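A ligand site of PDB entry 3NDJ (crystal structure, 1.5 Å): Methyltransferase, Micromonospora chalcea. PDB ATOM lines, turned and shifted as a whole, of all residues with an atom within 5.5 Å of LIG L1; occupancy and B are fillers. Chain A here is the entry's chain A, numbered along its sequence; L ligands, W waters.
Water W3 lies within hydrogen-bond range of an oxygen (O2) of LIG L1, the side-chain amide oxygen of Asn 179 and a ring nitrogen (NE2) of His 227.
Water W1 lies within hydrogen-bond range of OD1 of Asp 35 (2.7 Å), O8 of LIG L1 (2.8 Å) and NZ of Lys 355 (2.8 Å).
Water W4 lies within hydrogen-bond range of the side-chain hydroxyl of Tyr 325, a nitrogen (N3) of LIG L1 and the side-chain amino group of Lys 395.
Water W7 bridges OH of Tyr 224 (2.6 Å) and O1 of LIG L1 (3.0 Å).
Water W2 lies within hydrogen-bond range of O of Gly 84 (2.6 Å) and OG1 of Thr 351 (2.8 Å).
The side-chain carboxylate (OE1) of Glu 226 lies within salt-bridge range of a nitrogen (N1) of LIG L1.
NZ of Lys 355 is in hydrogen-bond range of O7 of LIG L1, at 2.7 Å.
OH of Tyr 80 is in hydrogen-bond range of O4 of LIG L1 (2.7 Å).
A ring nitrogen (NE2) of His 183 is in hydrogen-bond range of a nitrogen (N1) of LIG L1 (2.8 Å).
The side-chain hydroxyl of Thr 352 is in hydrogen-bond range of an oxygen (O7) of LIG L1.
O11 of LIG L1 lies within salt-bridge range of NZ of Lys 330, 2.9 Å away.
The side-chain amino group (NZ) of Lys 395 is in hydrogen-bond range of an oxygen (O10) of LIG L1, 2.8 Å away.
OH of Tyr 224 lies within hydrogen-bond range of N1 of LIG L1, 2.9 Å away.
O8 of LIG L1 is in hydrogen-bond range of N of Ala 329, at 2.8 Å.
An oxygen (O2) of LIG L1 is in hydrogen-bond range of a ring nitrogen (NE2) of His 227, at 2.8 Å.
OG1 of Thr 351 lies close to O5 of LIG L1 (3.3 Å).
O5 of LIG L1 is in hydrogen-bond range of N of Thr 351 (3.1 Å).
O1 of LG2 L2 lies within hydrogen-bond range of ND2 of Asn 179.
An oxygen (O6) of LIG L1 sits at hydrogen-bond distance from the side-chain amide nitrogen (ND2) of Asn 387, at 2.9 Å.
A ring nitrogen (NE2) of His 388 sits at hydrogen-bond distance from an oxygen (O4) of LIG L1 (2.8 Å).
An oxygen (O7) of LIG L1 sits at hydrogen-bond distance from the side-chain carboxylate (OD1) of Asp 350, at 2.7 Å.
Asp 35 touches LIG L1 (OD2 to C2, 3.9 Å).
OH of Tyr 78 touches C11 of LIG L1, at 3.2 Å.
Ser 85 touches LIG L1 (CB to C16, 3.999 Å).
CB of Asn 179 touches C6 of LIG L1 (3.7 Å).
His 256 touches LIG L1.
Gly 326 touches LIG L1 (CA to O9, 3.6 Å).
O of Ala 327 touches O7 of LIG L1 (3.8 Å).
Thr 328 touches LIG L1 (CA to O8, 3.3 Å).
Ala 385 touches LIG L1 (CB to O9, 3.999 Å).
Glu 391 touches LIG L1 (OE1 to C16, 3.6 Å).
Ile 392 touches LIG L1.
Hydrophobic or aromatic side chains within 4 Å of LIG L1: Tyr 80, His 183, Tyr 224, His 227, His 256, Ala 329, Ala 385, His 388 and Ile 392.
OE1 of Glu 391 is in hydrogen-bond range of N of Ser 86.
The backbone NH (N) of Ala 327 lies within hydrogen-bond range of the side-chain carboxylate (OD1) of Asp 350, 2.8 Å away.
OE1 of Glu 226 lies within hydrogen-bond range of OH of Tyr 78 (2.7 Å).
OE2 of Glu 226 lies close to OD2 of Asp 35.
The backbone NH (N) of Gly 326 is in hydrogen-bond range of the backbone carbonyl oxygen (O) of Tyr 349.
The side-chain hydroxyl (OH) of Tyr 224 sits at hydrogen-bond distance from a ring nitrogen (NE2) of His 227, 3.1 Å away.
A ring nitrogen (ND1) of His 256 is in hydrogen-bond range of the side-chain amide nitrogen (ND2) of Asn 387 (3.3 Å).
The side-chain hydroxyl of Thr 352 lies within hydrogen-bond range of the side-chain carboxylate of Asp 350 (2.7 Å).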
ATOM      1  N   ASP A  35     -10.028 -23.747  -1.245  1.00  0.00           N
ATOM      2  CA  ASP A  35     -11.331 -23.812  -0.591  1.00  0.00           C
ATOM      3  C   ASP A  35     -12.509 -23.310  -1.483  1.00  0.00           C
ATOM      4  O   ASP A  35     -13.593 -22.981  -0.958  1.00  0.00           O
ATOM      5  CB  ASP A  35     -11.290 -23.143   0.778  1.00  0.00           C
ATOM      6  CG  ASP A  35     -10.903 -24.107   1.894  1.00  0.00           C
ATOM      7  OD1 ASP A  35     -11.421 -25.225   1.967  1.00  0.00           O
ATOM      8  OD2 ASP A  35     -10.033 -23.677   2.692  1.00  0.00           O
ATOM      9  N   TYR A  78     -16.884 -18.830   2.562  1.00  0.00           N
ATOM     10  CA  TYR A  78     -15.758 -19.705   2.946  1.00  0.00           C
ATOM     11  C   TYR A  78     -16.286 -20.976   3.641  1.00  0.00           C
ATOM     12  O   TYR A  78     -17.116 -20.893   4.553  1.00  0.00           O
ATOM     13  CB  TYR A  78     -14.874 -18.945   3.951  1.00  0.00           C
ATOM     14  CG  TYR A  78     -13.633 -19.710   4.372  1.00  0.00           C
ATOM     15  CD1 TYR A  78     -13.487 -20.146   5.693  1.00  0.00           C
ATOM     16  CD2 TYR A  78     -12.622 -19.940   3.468  1.00  0.00           C
ATOM     17  CE1 TYR A  78     -12.338 -20.796   6.104  1.00  0.00           C
ATOM     18  CE2 TYR A  78     -11.470 -20.639   3.866  1.00  0.00           C
ATOM     19  CZ  TYR A  78     -11.359 -21.046   5.184  1.00  0.00           C
ATOM     20  OH  TYR A  78     -10.191 -21.690   5.585  1.00  0.00           O
ATOM     21  N   TYR A  80     -14.857 -23.896   5.368  1.00  0.00           N
ATOM     22  CA  TYR A  80     -14.331 -24.796   6.396  1.00  0.00           C
ATOM     23  C   TYR A  80     -15.043 -24.563   7.719  1.00  0.00           C
ATOM     24  O   TYR A  80     -15.167 -23.417   8.203  1.00  0.00           O
ATOM     25  CB  TYR A  80     -12.854 -24.490   6.670  1.00  0.00           C
ATOM     26  CG  TYR A  80     -12.261 -25.410   7.689  1.00  0.00           C
ATOM     27  CD1 TYR A  80     -12.161 -26.761   7.404  1.00  0.00           C
ATOM     28  CD2 TYR A  80     -11.772 -24.922   8.899  1.00  0.00           C
ATOM     29  CE1 TYR A  80     -11.580 -27.656   8.347  1.00  0.00           C
ATOM     30  CE2 TYR A  80     -11.220 -25.791   9.818  1.00  0.00           C
ATOM     31  CZ  TYR A  80     -11.117 -27.133   9.522  1.00  0.00           C
ATOM     32  OH  TYR A  80     -10.546 -27.980  10.418  1.00  0.00           O
ATOM     33  N   GLY A  84     -16.439 -29.384  12.777  1.00  0.00           N
ATOM     34  CA  GLY A  84     -16.737 -30.670  12.161  1.00  0.00           C
ATOM     35  C   GLY A  84     -15.884 -31.784  12.725  1.00  0.00           C
ATOM     36  O   GLY A  84     -16.096 -32.972  12.411  1.00  0.00           O
ATOM     37  N   SER A  85     -14.927 -31.457  13.581  1.00  0.00           N
ATOM     38  CA  SER A  85     -14.029 -32.465  14.160  1.00  0.00           C
ATOM     39  C   SER A  85     -14.187 -32.565  15.677  1.00  0.00           C
ATOM     40  O   SER A  85     -14.088 -31.566  16.378  1.00  0.00           O
ATOM     41  CB  SER A  85     -12.541 -32.166  13.913  1.00  0.00           C
ATOM     42  OG  SER A  85     -11.701 -32.918  14.807  1.00  0.00           O
ATOM     43  N   SER A  86     -14.404 -33.774  16.195  1.00  0.00           N
ATOM     44  CA  SER A  86     -14.575 -33.924  17.647  1.00  0.00           C
ATOM     45  C   SER A  86     -13.265 -33.741  18.434  1.00  0.00           C
ATOM     46  O   SER A  86     -13.249 -33.108  19.502  1.00  0.00           O
ATOM     47  CB  SER A  86     -15.225 -35.269  17.955  1.00  0.00           C
ATOM     48  OG  SER A  86     -14.310 -36.356  17.671  1.00  0.00           O
ATOM     49  N   ASN A 179      -4.397 -21.855  13.530  1.00  0.00           N
ATOM     50  CA  ASN A 179      -4.562 -22.026  12.069  1.00  0.00           C
ATOM     51  C   ASN A 179      -5.060 -20.775  11.354  1.00  0.00           C
ATOM     52  O   ASN A 179      -5.881 -20.882  10.436  1.00  0.00           O
ATOM     53  CB  ASN A 179      -5.505 -23.196  11.836  1.00  0.00           C
ATOM     54  CG  ASN A 179      -5.048 -24.375  12.675  1.00  0.00           C
ATOM     55  OD1 ASN A 179      -3.941 -24.878  12.443  1.00  0.00           O
ATOM     56  ND2 ASN A 179      -5.866 -24.770  13.648  1.00  0.00           N
ATOM     57  N   HIS A 183      -1.773 -17.845   7.898  1.00  0.00           N
ATOM     58  CA  HIS A 183      -2.568 -17.542   6.711  1.00  0.00           C
ATOM     59  C   HIS A 183      -2.393 -16.084   6.271  1.00  0.00           C
ATOM     60  O   HIS A 183      -2.898 -15.796   5.203  1.00  0.00           O
ATOM     61  CB  HIS A 183      -4.053 -17.755   7.004  1.00  0.00           C
ATOM     62  CG  HIS A 183      -4.428 -19.190   7.270  1.00  0.00           C
ATOM     63  ND1 HIS A 183      -3.682 -20.024   8.080  1.00  0.00           N
ATOM     64  CD2 HIS A 183      -5.468 -19.946   6.833  1.00  0.00           C
ATOM     65  CE1 HIS A 183      -4.226 -21.224   8.114  1.00  0.00           C
ATOM     66  NE2 HIS A 183      -5.318 -21.203   7.376  1.00  0.00           N
ATOM     67  N   TYR A 224      -0.324 -24.641   0.560  1.00  0.00           N
ATOM     68  CA  TYR A 224      -1.407 -24.313  -0.360  1.00  0.00           C
ATOM     69  C   TYR A 224      -1.728 -22.826  -0.131  1.00  0.00           C
ATOM     70  O   TYR A 224      -1.056 -22.230   0.698  1.00  0.00           O
ATOM     71  CB  TYR A 224      -2.628 -25.222  -0.191  1.00  0.00           C
ATOM     72  CG  TYR A 224      -3.300 -25.296   1.158  1.00  0.00           C
ATOM     73  CD1 TYR A 224      -4.410 -24.461   1.424  1.00  0.00           C
ATOM     74  CD2 TYR A 224      -2.860 -26.161   2.165  1.00  0.00           C
ATOM     75  CE1 TYR A 224      -5.076 -24.506   2.619  1.00  0.00           C
ATOM     76  CE2 TYR A 224      -3.516 -26.218   3.342  1.00  0.00           C
ATOM     77  CZ  TYR A 224      -4.606 -25.373   3.613  1.00  0.00           C
ATOM     78  OH  TYR A 224      -5.256 -25.480   4.807  1.00  0.00           O
ATOM     79  N   GLU A 226      -3.684 -20.807   1.397  1.00  0.00           N
ATOM     80  CA  GLU A 226      -3.995 -20.250   2.721  1.00  0.00           C
ATOM     81  C   GLU A 226      -2.850 -20.457   3.712  1.00  0.00           C
ATOM     82  O   GLU A 226      -2.897 -19.881   4.829  1.00  0.00           O
ATOM     83  CB  GLU A 226      -5.221 -20.939   3.331  1.00  0.00           C
ATOM     84  CG  GLU A 226      -6.491 -20.597   2.487  1.00  0.00           C
ATOM     85  CD  GLU A 226      -7.702 -21.350   2.962  1.00  0.00           C
ATOM     86  OE1 GLU A 226      -7.856 -21.682   4.170  1.00  0.00           O
ATOM     87  OE2 GLU A 226      -8.581 -21.620   2.108  1.00  0.00           O
ATOM     88  N   HIS A 227      -1.855 -21.294   3.386  1.00  0.00           N
ATOM     89  CA  HIS A 227      -0.776 -21.331   4.324  1.00  0.00           C
ATOM     90  C   HIS A 227       0.420 -20.557   3.798  1.00  0.00           C
ATOM     91  O   HIS A 227       1.303 -21.104   3.131  1.00  0.00           O
ATOM     92  CB  HIS A 227      -0.396 -22.800   4.531  1.00  0.00           C
ATOM     93  CG  HIS A 227      -1.400 -23.529   5.372  1.00  0.00           C
ATOM     94  ND1 HIS A 227      -1.273 -24.876   5.655  1.00  0.00           N
ATOM     95  CD2 HIS A 227      -2.547 -23.126   5.991  1.00  0.00           C
ATOM     96  CE1 HIS A 227      -2.292 -25.266   6.400  1.00  0.00           C
ATOM     97  NE2 HIS A 227      -3.058 -24.222   6.640  1.00  0.00           N
ATOM     98  N   HIS A 256      -3.624 -31.376  13.293  1.00  0.00           N
ATOM     99  CA  HIS A 256      -3.316 -30.872  11.958  1.00  0.00           C
ATOM    100  C   HIS A 256      -1.965 -31.274  11.385  1.00  0.00           C
ATOM    101  O   HIS A 256      -1.305 -30.484  10.723  1.00  0.00           O
ATOM    102  CB  HIS A 256      -3.515 -29.374  11.870  1.00  0.00           C
ATOM    103  CG  HIS A 256      -4.956 -29.019  11.965  1.00  0.00           C
ATOM    104  ND1 HIS A 256      -5.884 -29.463  11.037  1.00  0.00           N
ATOM    105  CD2 HIS A 256      -5.651 -28.303  12.880  1.00  0.00           C
ATOM    106  CE1 HIS A 256      -7.080 -29.025  11.389  1.00  0.00           C
ATOM    107  NE2 HIS A 256      -6.967 -28.316  12.490  1.00  0.00           N
ATOM    108  N   TYR A 325     -11.148 -39.595   0.909  1.00  0.00           N
ATOM    109  CA  TYR A 325     -11.873 -39.329   2.116  1.00  0.00           C
ATOM    110  C   TYR A 325     -11.301 -38.105   2.771  1.00  0.00           C
ATOM    111  O   TYR A 325     -10.149 -38.002   3.166  1.00  0.00           O
ATOM    112  CB  TYR A 325     -11.788 -40.535   3.016  1.00  0.00           C
ATOM    113  CG  TYR A 325     -12.873 -40.580   4.046  1.00  0.00           C
ATOM    114  CD1 TYR A 325     -13.009 -39.545   4.980  1.00  0.00           C
ATOM    115  CD2 TYR A 325     -13.787 -41.665   4.053  1.00  0.00           C
ATOM    116  CE1 TYR A 325     -14.022 -39.600   5.953  1.00  0.00           C
ATOM    117  CE2 TYR A 325     -14.807 -41.703   5.020  1.00  0.00           C
ATOM    118  CZ  TYR A 325     -14.895 -40.691   5.955  1.00  0.00           C
ATOM    119  OH  TYR A 325     -15.915 -40.739   6.896  1.00  0.00           O
ATOM    120  N   GLY A 326     -12.175 -37.101   2.769  1.00  0.00           N
ATOM    121  CA  GLY A 326     -12.004 -35.759   3.343  1.00  0.00           C
ATOM    122  C   GLY A 326     -11.690 -34.791   2.214  1.00  0.00           C
ATOM    123  O   GLY A 326     -10.666 -34.870   1.564  1.00  0.00           O
ATOM    124  N   ALA A 327     -12.591 -33.841   1.961  1.00  0.00           N
ATOM    125  CA  ALA A 327     -12.384 -32.778   0.940  1.00  0.00           C
ATOM    126  C   ALA A 327     -11.593 -31.607   1.532  1.00  0.00           C
ATOM    127  O   ALA A 327     -12.040 -30.436   1.668  1.00  0.00           O
ATOM    128  CB  ALA A 327     -13.729 -32.248   0.368  1.00  0.00           C
ATOM    129  N   THR A 328     -10.380 -31.931   1.941  1.00  0.00           N
ATOM    130  CA  THR A 328      -9.493 -31.000   2.609  1.00  0.00           C
ATOM    131  C   THR A 328      -9.053 -29.902   1.660  1.00  0.00           C
ATOM    132  O   THR A 328      -8.943 -30.132   0.475  1.00  0.00           O
ATOM    133  CB  THR A 328      -8.215 -31.717   3.157  1.00  0.00           C
ATOM    134  OG1 THR A 328      -7.564 -32.344   2.060  1.00  0.00           O
ATOM    135  CG2 THR A 328      -8.564 -32.741   4.268  1.00  0.00           C
ATOM    136  N   ALA A 329      -8.780 -28.730   2.211  1.00  0.00           N
ATOM    137  CA  ALA A 329      -8.022 -27.735   1.456  1.00  0.00           C
ATOM    138  C   ALA A 329      -6.668 -28.305   0.986  1.00  0.00           C
ATOM    139  O   ALA A 329      -6.283 -28.082  -0.131  1.00  0.00           O
ATOM    140  CB  ALA A 329      -7.846 -26.484   2.323  1.00  0.00           C
ATOM    141  N   LYS A 330      -6.016 -29.018   1.903  1.00  0.00           N
ATOM    142  CA  LYS A 330      -4.725 -29.620   1.617  1.00  0.00           C
ATOM    143  C   LYS A 330      -4.778 -30.445   0.339  1.00  0.00           C
ATOM    144  O   LYS A 330      -3.803 -30.438  -0.430  1.00  0.00           O
ATOM    145  CB  LYS A 330      -4.391 -30.600   2.754  1.00  0.00           C
ATOM    146  CG  LYS A 330      -4.019 -29.870   4.081  1.00  0.00           C
ATOM    147  CD  LYS A 330      -3.424 -30.820   5.141  1.00  0.00           C
ATOM    148  CE  LYS A 330      -4.364 -31.945   5.588  1.00  0.00           C
ATOM    149  NZ  LYS A 330      -5.448 -31.397   6.411  1.00  0.00           N
ATOM    150  N   TYR A 349     -15.388 -38.120  -0.192  1.00  0.00           N
ATOM    151  CA  TYR A 349     -16.456 -38.124   0.801  1.00  0.00           C
ATOM    152  C   TYR A 349     -16.147 -37.131   1.909  1.00  0.00           C
ATOM    153  O   TYR A 349     -15.007 -36.979   2.363  1.00  0.00           O
ATOM    154  CB  TYR A 349     -16.618 -39.548   1.387  1.00  0.00           C
ATOM    155  CG  TYR A 349     -17.120 -40.416   0.287  1.00  0.00           C
ATOM    156  CD1 TYR A 349     -18.461 -40.443  -0.047  1.00  0.00           C
ATOM    157  CD2 TYR A 349     -16.249 -41.149  -0.503  1.00  0.00           C
ATOM    158  CE1 TYR A 349     -18.958 -41.194  -1.113  1.00  0.00           C
ATOM    159  CE2 TYR A 349     -16.713 -41.898  -1.539  1.00  0.00           C
ATOM    160  CZ  TYR A 349     -18.063 -41.947  -1.827  1.00  0.00           C
ATOM    161  OH  TYR A 349     -18.419 -42.704  -2.890  1.00  0.00           O
ATOM    162  N   ASP A 350     -17.145 -36.351   2.337  1.00  0.00           N
ATOM    163  CA  ASP A 350     -16.860 -35.259   3.268  1.00  0.00           C
ATOM    164  C   ASP A 350     -18.113 -34.818   4.061  1.00  0.00           C
ATOM    165  O   ASP A 350     -19.208 -34.885   3.502  1.00  0.00           O
ATOM    166  CB  ASP A 350     -16.408 -34.015   2.492  1.00  0.00           C
ATOM    167  CG  ASP A 350     -15.852 -32.936   3.407  1.00  0.00           C
ATOM    168  OD1 ASP A 350     -14.619 -32.952   3.657  1.00  0.00           O
ATOM    169  OD2 ASP A 350     -16.624 -32.060   3.862  1.00  0.00           O
ATOM    170  N   THR A 351     -17.944 -34.448   5.333  1.00  0.00           N
ATOM    171  CA  THR A 351     -19.056 -34.192   6.242  1.00  0.00           C
ATOM    172  C   THR A 351     -19.602 -32.778   6.181  1.00  0.00           C
ATOM    173  O   THR A 351     -20.542 -32.474   6.910  1.00  0.00           O
ATOM    174  CB  THR A 351     -18.728 -34.442   7.701  1.00  0.00           C
ATOM    175  OG1 THR A 351     -17.480 -33.816   7.997  1.00  0.00           O
ATOM    176  CG2 THR A 351     -18.590 -35.960   7.908  1.00  0.00           C
ATOM    177  N   THR A 352     -18.972 -31.969   5.348  1.00  0.00           N
ATOM    178  CA  THR A 352     -19.344 -30.552   5.212  1.00  0.00           C
ATOM    179  C   THR A 352     -20.454 -30.245   4.202  1.00  0.00           C
ATOM    180  O   THR A 352     -20.262 -30.399   2.999  1.00  0.00           O
ATOM    181  CB  THR A 352     -18.125 -29.672   4.829  1.00  0.00           C
ATOM    182  OG1 THR A 352     -16.969 -30.021   5.599  1.00  0.00           O
ATOM    183  CG2 THR A 352     -18.402 -28.178   5.123  1.00  0.00           C
ATOM    184  N   LYS A 355     -19.591 -28.300   1.020  1.00  0.00           N
ATOM    185  CA  LYS A 355     -18.694 -28.944   0.057  1.00  0.00           C
ATOM    186  C   LYS A 355     -19.334 -30.110  -0.707  1.00  0.00           C
ATOM    187  O   LYS A 355     -18.841 -30.494  -1.762  1.00  0.00           O
ATOM    188  CB  LYS A 355     -17.392 -29.448   0.725  1.00  0.00           C
ATOM    189  CG  LYS A 355     -16.533 -28.392   1.492  1.00  0.00           C
ATOM    190  CD  LYS A 355     -15.340 -29.054   2.139  1.00  0.00           C
ATOM    191  CE  LYS A 355     -14.493 -28.030   2.894  1.00  0.00           C
ATOM    192  NZ  LYS A 355     -13.298 -28.765   3.462  1.00  0.00           N
ATOM    193  N   ALA A 370     -20.246 -37.833   3.544  1.00  0.00           N
ATOM    194  CA  ALA A 370     -19.618 -39.030   4.121  1.00  0.00           C
ATOM    195  C   ALA A 370     -20.597 -40.155   4.389  1.00  0.00           C
ATOM    196  O   ALA A 370     -20.198 -41.330   4.396  1.00  0.00           O
ATOM    197  CB  ALA A 370     -18.884 -38.623   5.383  1.00  0.00           C
ATOM    198  N   ALA A 385      -7.822 -36.506   4.535  1.00  0.00           N
ATOM    199  CA  ALA A 385      -7.914 -36.031   5.941  1.00  0.00           C
ATOM    200  C   ALA A 385      -7.032 -36.879   6.869  1.00  0.00           C
ATOM    201  O   ALA A 385      -7.501 -37.381   7.918  1.00  0.00           O
ATOM    202  CB  ALA A 385      -9.371 -36.026   6.398  1.00  0.00           C
ATOM    203  N   ASN A 387      -4.711 -36.124   8.847  1.00  0.00           N
ATOM    204  CA  ASN A 387      -4.556 -35.601  10.179  1.00  0.00           C
ATOM    205  C   ASN A 387      -5.684 -35.949  11.149  1.00  0.00           C
ATOM    206  O   ASN A 387      -5.550 -35.712  12.347  1.00  0.00           O
ATOM    207  CB  ASN A 387      -4.419 -34.082  10.092  1.00  0.00           C
ATOM    208  CG  ASN A 387      -5.542 -33.455   9.292  1.00  0.00           C
ATOM    209  OD1 ASN A 387      -5.659 -33.825   8.117  1.00  0.00           O
ATOM    210  ND2 ASN A 387      -6.329 -32.519   9.869  1.00  0.00           N
ATOM    211  N   HIS A 388      -6.764 -36.512  10.629  1.00  0.00           N
ATOM    212  CA  HIS A 388      -7.946 -36.914  11.378  1.00  0.00           C
ATOM    213  C   HIS A 388      -8.058 -38.439  11.287  1.00  0.00           C
ATOM    214  O   HIS A 388      -9.151 -38.952  11.514  1.00  0.00           O
ATOM    215  CB  HIS A 388      -9.197 -36.305  10.719  1.00  0.00           C
ATOM    216  CG  HIS A 388      -9.312 -34.822  10.875  1.00  0.00           C
ATOM    217  ND1 HIS A 388      -9.418 -34.229  12.113  1.00  0.00           N
ATOM    218  CD2 HIS A 388      -9.260 -33.815   9.956  1.00  0.00           C
ATOM    219  CE1 HIS A 388      -9.513 -32.905  11.952  1.00  0.00           C
ATOM    220  NE2 HIS A 388      -9.390 -32.639  10.661  1.00  0.00           N
ATOM    221  N   GLU A 391      -9.883 -40.429  14.294  1.00  0.00           N
ATOM    222  CA  GLU A 391     -11.278 -39.982  14.432  1.00  0.00           C
ATOM    223  C   GLU A 391     -12.130 -40.537  13.289  1.00  0.00           C
ATOM    224  O   GLU A 391     -13.212 -41.081  13.511  1.00  0.00           O
ATOM    225  CB  GLU A 391     -11.382 -38.448  14.361  1.00  0.00           C
ATOM    226  CG  GLU A 391     -12.804 -37.934  14.558  1.00  0.00           C
ATOM    227  CD  GLU A 391     -12.930 -36.429  14.692  1.00  0.00           C
ATOM    228  OE1 GLU A 391     -14.087 -35.957  14.508  1.00  0.00           O
ATOM    229  OE2 GLU A 391     -11.942 -35.731  15.030  1.00  0.00           O
ATOM    230  N   ILE A 392     -11.622 -40.411  12.064  1.00  0.00           N
ATOM    231  CA  ILE A 392     -12.253 -41.049  10.898  1.00  0.00           C
ATOM    232  C   ILE A 392     -12.276 -42.586  10.924  1.00  0.00           C
ATOM    233  O   ILE A 392     -13.319 -43.223  10.700  1.00  0.00           O
ATOM    234  CB  ILE A 392     -11.607 -40.484   9.581  1.00  0.00           C
ATOM    235  CG1 ILE A 392     -11.970 -39.013   9.389  1.00  0.00           C
ATOM    236  CG2 ILE A 392     -12.134 -41.283   8.382  1.00  0.00           C
ATOM    237  CD1 ILE A 392     -11.280 -38.314   8.168  1.00  0.00           C
ATOM    238  N   LYS A 395     -14.907 -44.019  13.060  1.00  0.00           N
ATOM    239  CA  LYS A 395     -16.268 -43.982  12.540  1.00  0.00           C
ATOM    240  C   LYS A 395     -16.417 -44.857  11.309  1.00  0.00           C
ATOM    241  O   LYS A 395     -17.527 -45.021  10.815  1.00  0.00           O
ATOM    242  CB  LYS A 395     -16.634 -42.559  12.117  1.00  0.00           C
ATOM    243  CG  LYS A 395     -16.597 -41.646  13.304  1.00  0.00           C
ATOM    244  CD  LYS A 395     -17.293 -40.378  12.950  1.00  0.00           C
ATOM    245  CE  LYS A 395     -16.274 -39.485  12.298  1.00  0.00           C
ATOM    246  NZ  LYS A 395     -17.004 -38.311  11.751  1.00  0.00           N
HETATM  247  P1  LIG L   1      -9.124 -30.508   7.906  1.00  0.00           P
HETATM  248  C1  LIG L   1      -8.789 -26.173   6.644  1.00  0.00           C
HETATM  249  O1  LIG L   1      -7.808 -27.045   6.106  1.00  0.00           O
HETATM  250  C2  LIG L   1      -8.500 -24.760   6.063  1.00  0.00           C
HETATM  251  P2  LIG L   1      -8.264 -28.558   5.822  1.00  0.00           P
HETATM  252  C3  LIG L   1      -7.493 -23.973   6.924  1.00  0.00           C
HETATM  253  N1  LIG L   1      -6.631 -23.212   6.026  1.00  0.00           N
HETATM  254  C4  LIG L   1      -6.662 -24.883   7.806  1.00  0.00           C
HETATM  255  O2  LIG L   1      -5.454 -24.748   8.026  1.00  0.00           O
HETATM  256  C5  LIG L   1      -7.300 -26.011   8.556  1.00  0.00           C
HETATM  257  O3  LIG L   1      -8.635 -26.075   8.041  1.00  0.00           O
HETATM  258  C6  LIG L   1      -7.350 -25.828  10.057  1.00  0.00           C
HETATM  259  C7  LIG L   1     -13.827 -33.675   6.593  1.00  0.00           C
HETATM  260  N2  LIG L   1     -14.028 -34.651   7.689  1.00  0.00           N
HETATM  261  O4  LIG L   1      -9.675 -30.226   9.265  1.00  0.00           O
HETATM  262  C8  LIG L   1     -14.245 -32.284   7.028  1.00  0.00           C
HETATM  263  C9  LIG L   1     -14.853 -35.694   7.509  1.00  0.00           C
HETATM  264  O5  LIG L   1     -15.451 -35.894   6.438  1.00  0.00           O
HETATM  265  O6  LIG L   1      -8.052 -31.567   7.800  1.00  0.00           O
HETATM  266  C10 LIG L   1     -13.259 -31.335   6.349  1.00  0.00           C
HETATM  267  O7  LIG L   1     -13.730 -30.856   5.065  1.00  0.00           O
HETATM  268  N3  LIG L   1     -15.019 -36.598   8.505  1.00  0.00           N
HETATM  269  C11 LIG L   1      -8.201 -22.913   7.825  1.00  0.00           C
HETATM  270  O8  LIG L   1      -9.444 -28.571   4.901  1.00  0.00           O
HETATM  271  C12 LIG L   1     -12.015 -32.190   6.121  1.00  0.00           C
HETATM  272  O9  LIG L   1     -12.482 -33.524   6.164  1.00  0.00           O
HETATM  273  C13 LIG L   1     -14.453 -36.393   9.694  1.00  0.00           C
HETATM  274  O10 LIG L   1     -14.670 -37.336  10.643  1.00  0.00           O
HETATM  275  O11 LIG L   1      -7.072 -29.254   5.261  1.00  0.00           O
HETATM  276  C14 LIG L   1     -10.898 -32.156   7.147  1.00  0.00           C
HETATM  277  O12 LIG L   1     -10.290 -30.907   6.879  1.00  0.00           O
HETATM  278  C15 LIG L   1     -13.590 -35.348   9.932  1.00  0.00           C
HETATM  279  C16 LIG L   1     -12.864 -35.106  11.222  1.00  0.00           C
HETATM  280  C17 LIG L   1     -13.380 -34.487   8.855  1.00  0.00           C
HETATM  281  O13 LIG L   1      -8.720 -29.072   7.280  1.00  0.00           O
HETATM  282  N1  LG2 L   2      -9.256 -21.206  14.571  1.00  0.00           N
HETATM  283  C1  LG2 L   2     -10.088 -22.025  13.662  1.00  0.00           C
HETATM  284  C2  LG2 L   2     -10.243 -21.271  12.343  1.00  0.00           C
HETATM  285  C3  LG2 L   2      -9.522 -21.976  11.199  1.00  0.00           C
HETATM  286  S1  LG2 L   2     -10.079 -21.325   9.660  1.00  0.00           S
HETATM  287  C4  LG2 L   2      -9.374 -23.341  13.727  1.00  0.00           C
HETATM  288  O1  LG2 L   2      -8.243 -23.354  14.208  1.00  0.00           O
HETATM  289  O2  LG2 L   2     -10.017 -24.288  13.298  1.00  0.00           O
HETATM  290  C5  LG2 L   2      -9.120 -19.847   9.478  1.00  0.00           C
HETATM  291  C6  LG2 L   2     -10.026 -18.632   9.628  1.00  0.00           C
HETATM  292  O3  LG2 L   2      -9.141 -17.505   9.583  1.00  0.00           O
HETATM  293  C7  LG2 L   2     -11.056 -18.416   8.485  1.00  0.00           C
HETATM  294  O4  LG2 L   2     -12.355 -18.514   9.075  1.00  0.00           O
HETATM  295  C8  LG2 L   2     -10.748 -17.038   7.946  1.00  0.00           C
HETATM  296  O5  LG2 L   2     -11.919 -16.272   7.600  1.00  0.00           O
HETATM  297  C9  LG2 L   2     -10.008 -16.434   9.139  1.00  0.00           C
HETATM  298  N2  LG2 L   2      -9.131 -15.294   8.783  1.00  0.00           N
HETATM  299  C10 LG2 L   2      -8.373 -15.051   7.713  1.00  0.00           C
HETATM  300  N3  LG2 L   2      -7.652 -13.917   7.726  1.00  0.00           N
HETATM  301  C11 LG2 L   2      -8.014 -13.369   8.926  1.00  0.00           C
HETATM  302  C12 LG2 L   2      -7.646 -12.167   9.707  1.00  0.00           C
HETATM  303  N4  LG2 L   2      -6.797 -11.268   9.120  1.00  0.00           N
HETATM  304  N5  LG2 L   2      -8.272 -12.026  10.890  1.00  0.00           N
HETATM  305  C13 LG2 L   2      -9.105 -12.892  11.518  1.00  0.00           C
HETATM  306  N6  LG2 L   2      -9.500 -13.981  10.863  1.00  0.00           N
HETATM  307  C14 LG2 L   2      -8.947 -14.279   9.651  1.00  0.00           C
HETATM  308  O   HOH W   1     -11.448 -26.777   4.178  1.00  0.00           O
HETATM  309  O   HOH W   2     -17.065 -34.625  10.602  1.00  0.00           O
HETATM  310  O   HOH W   3      -3.550 -25.526   9.780  1.00  0.00           O
HETATM  311  O   HOH W   4     -16.850 -38.727   8.438  1.00  0.00           O
HETATM  312  O   HOH W   5     -12.801 -31.221  10.160  1.00  0.00           O
HETATM  313  O   HOH W   6     -14.890 -29.633   9.119  1.00  0.00           O
HETATM  314  O   HOH W   7      -4.806 -27.488   6.333  1.00  0.00           O
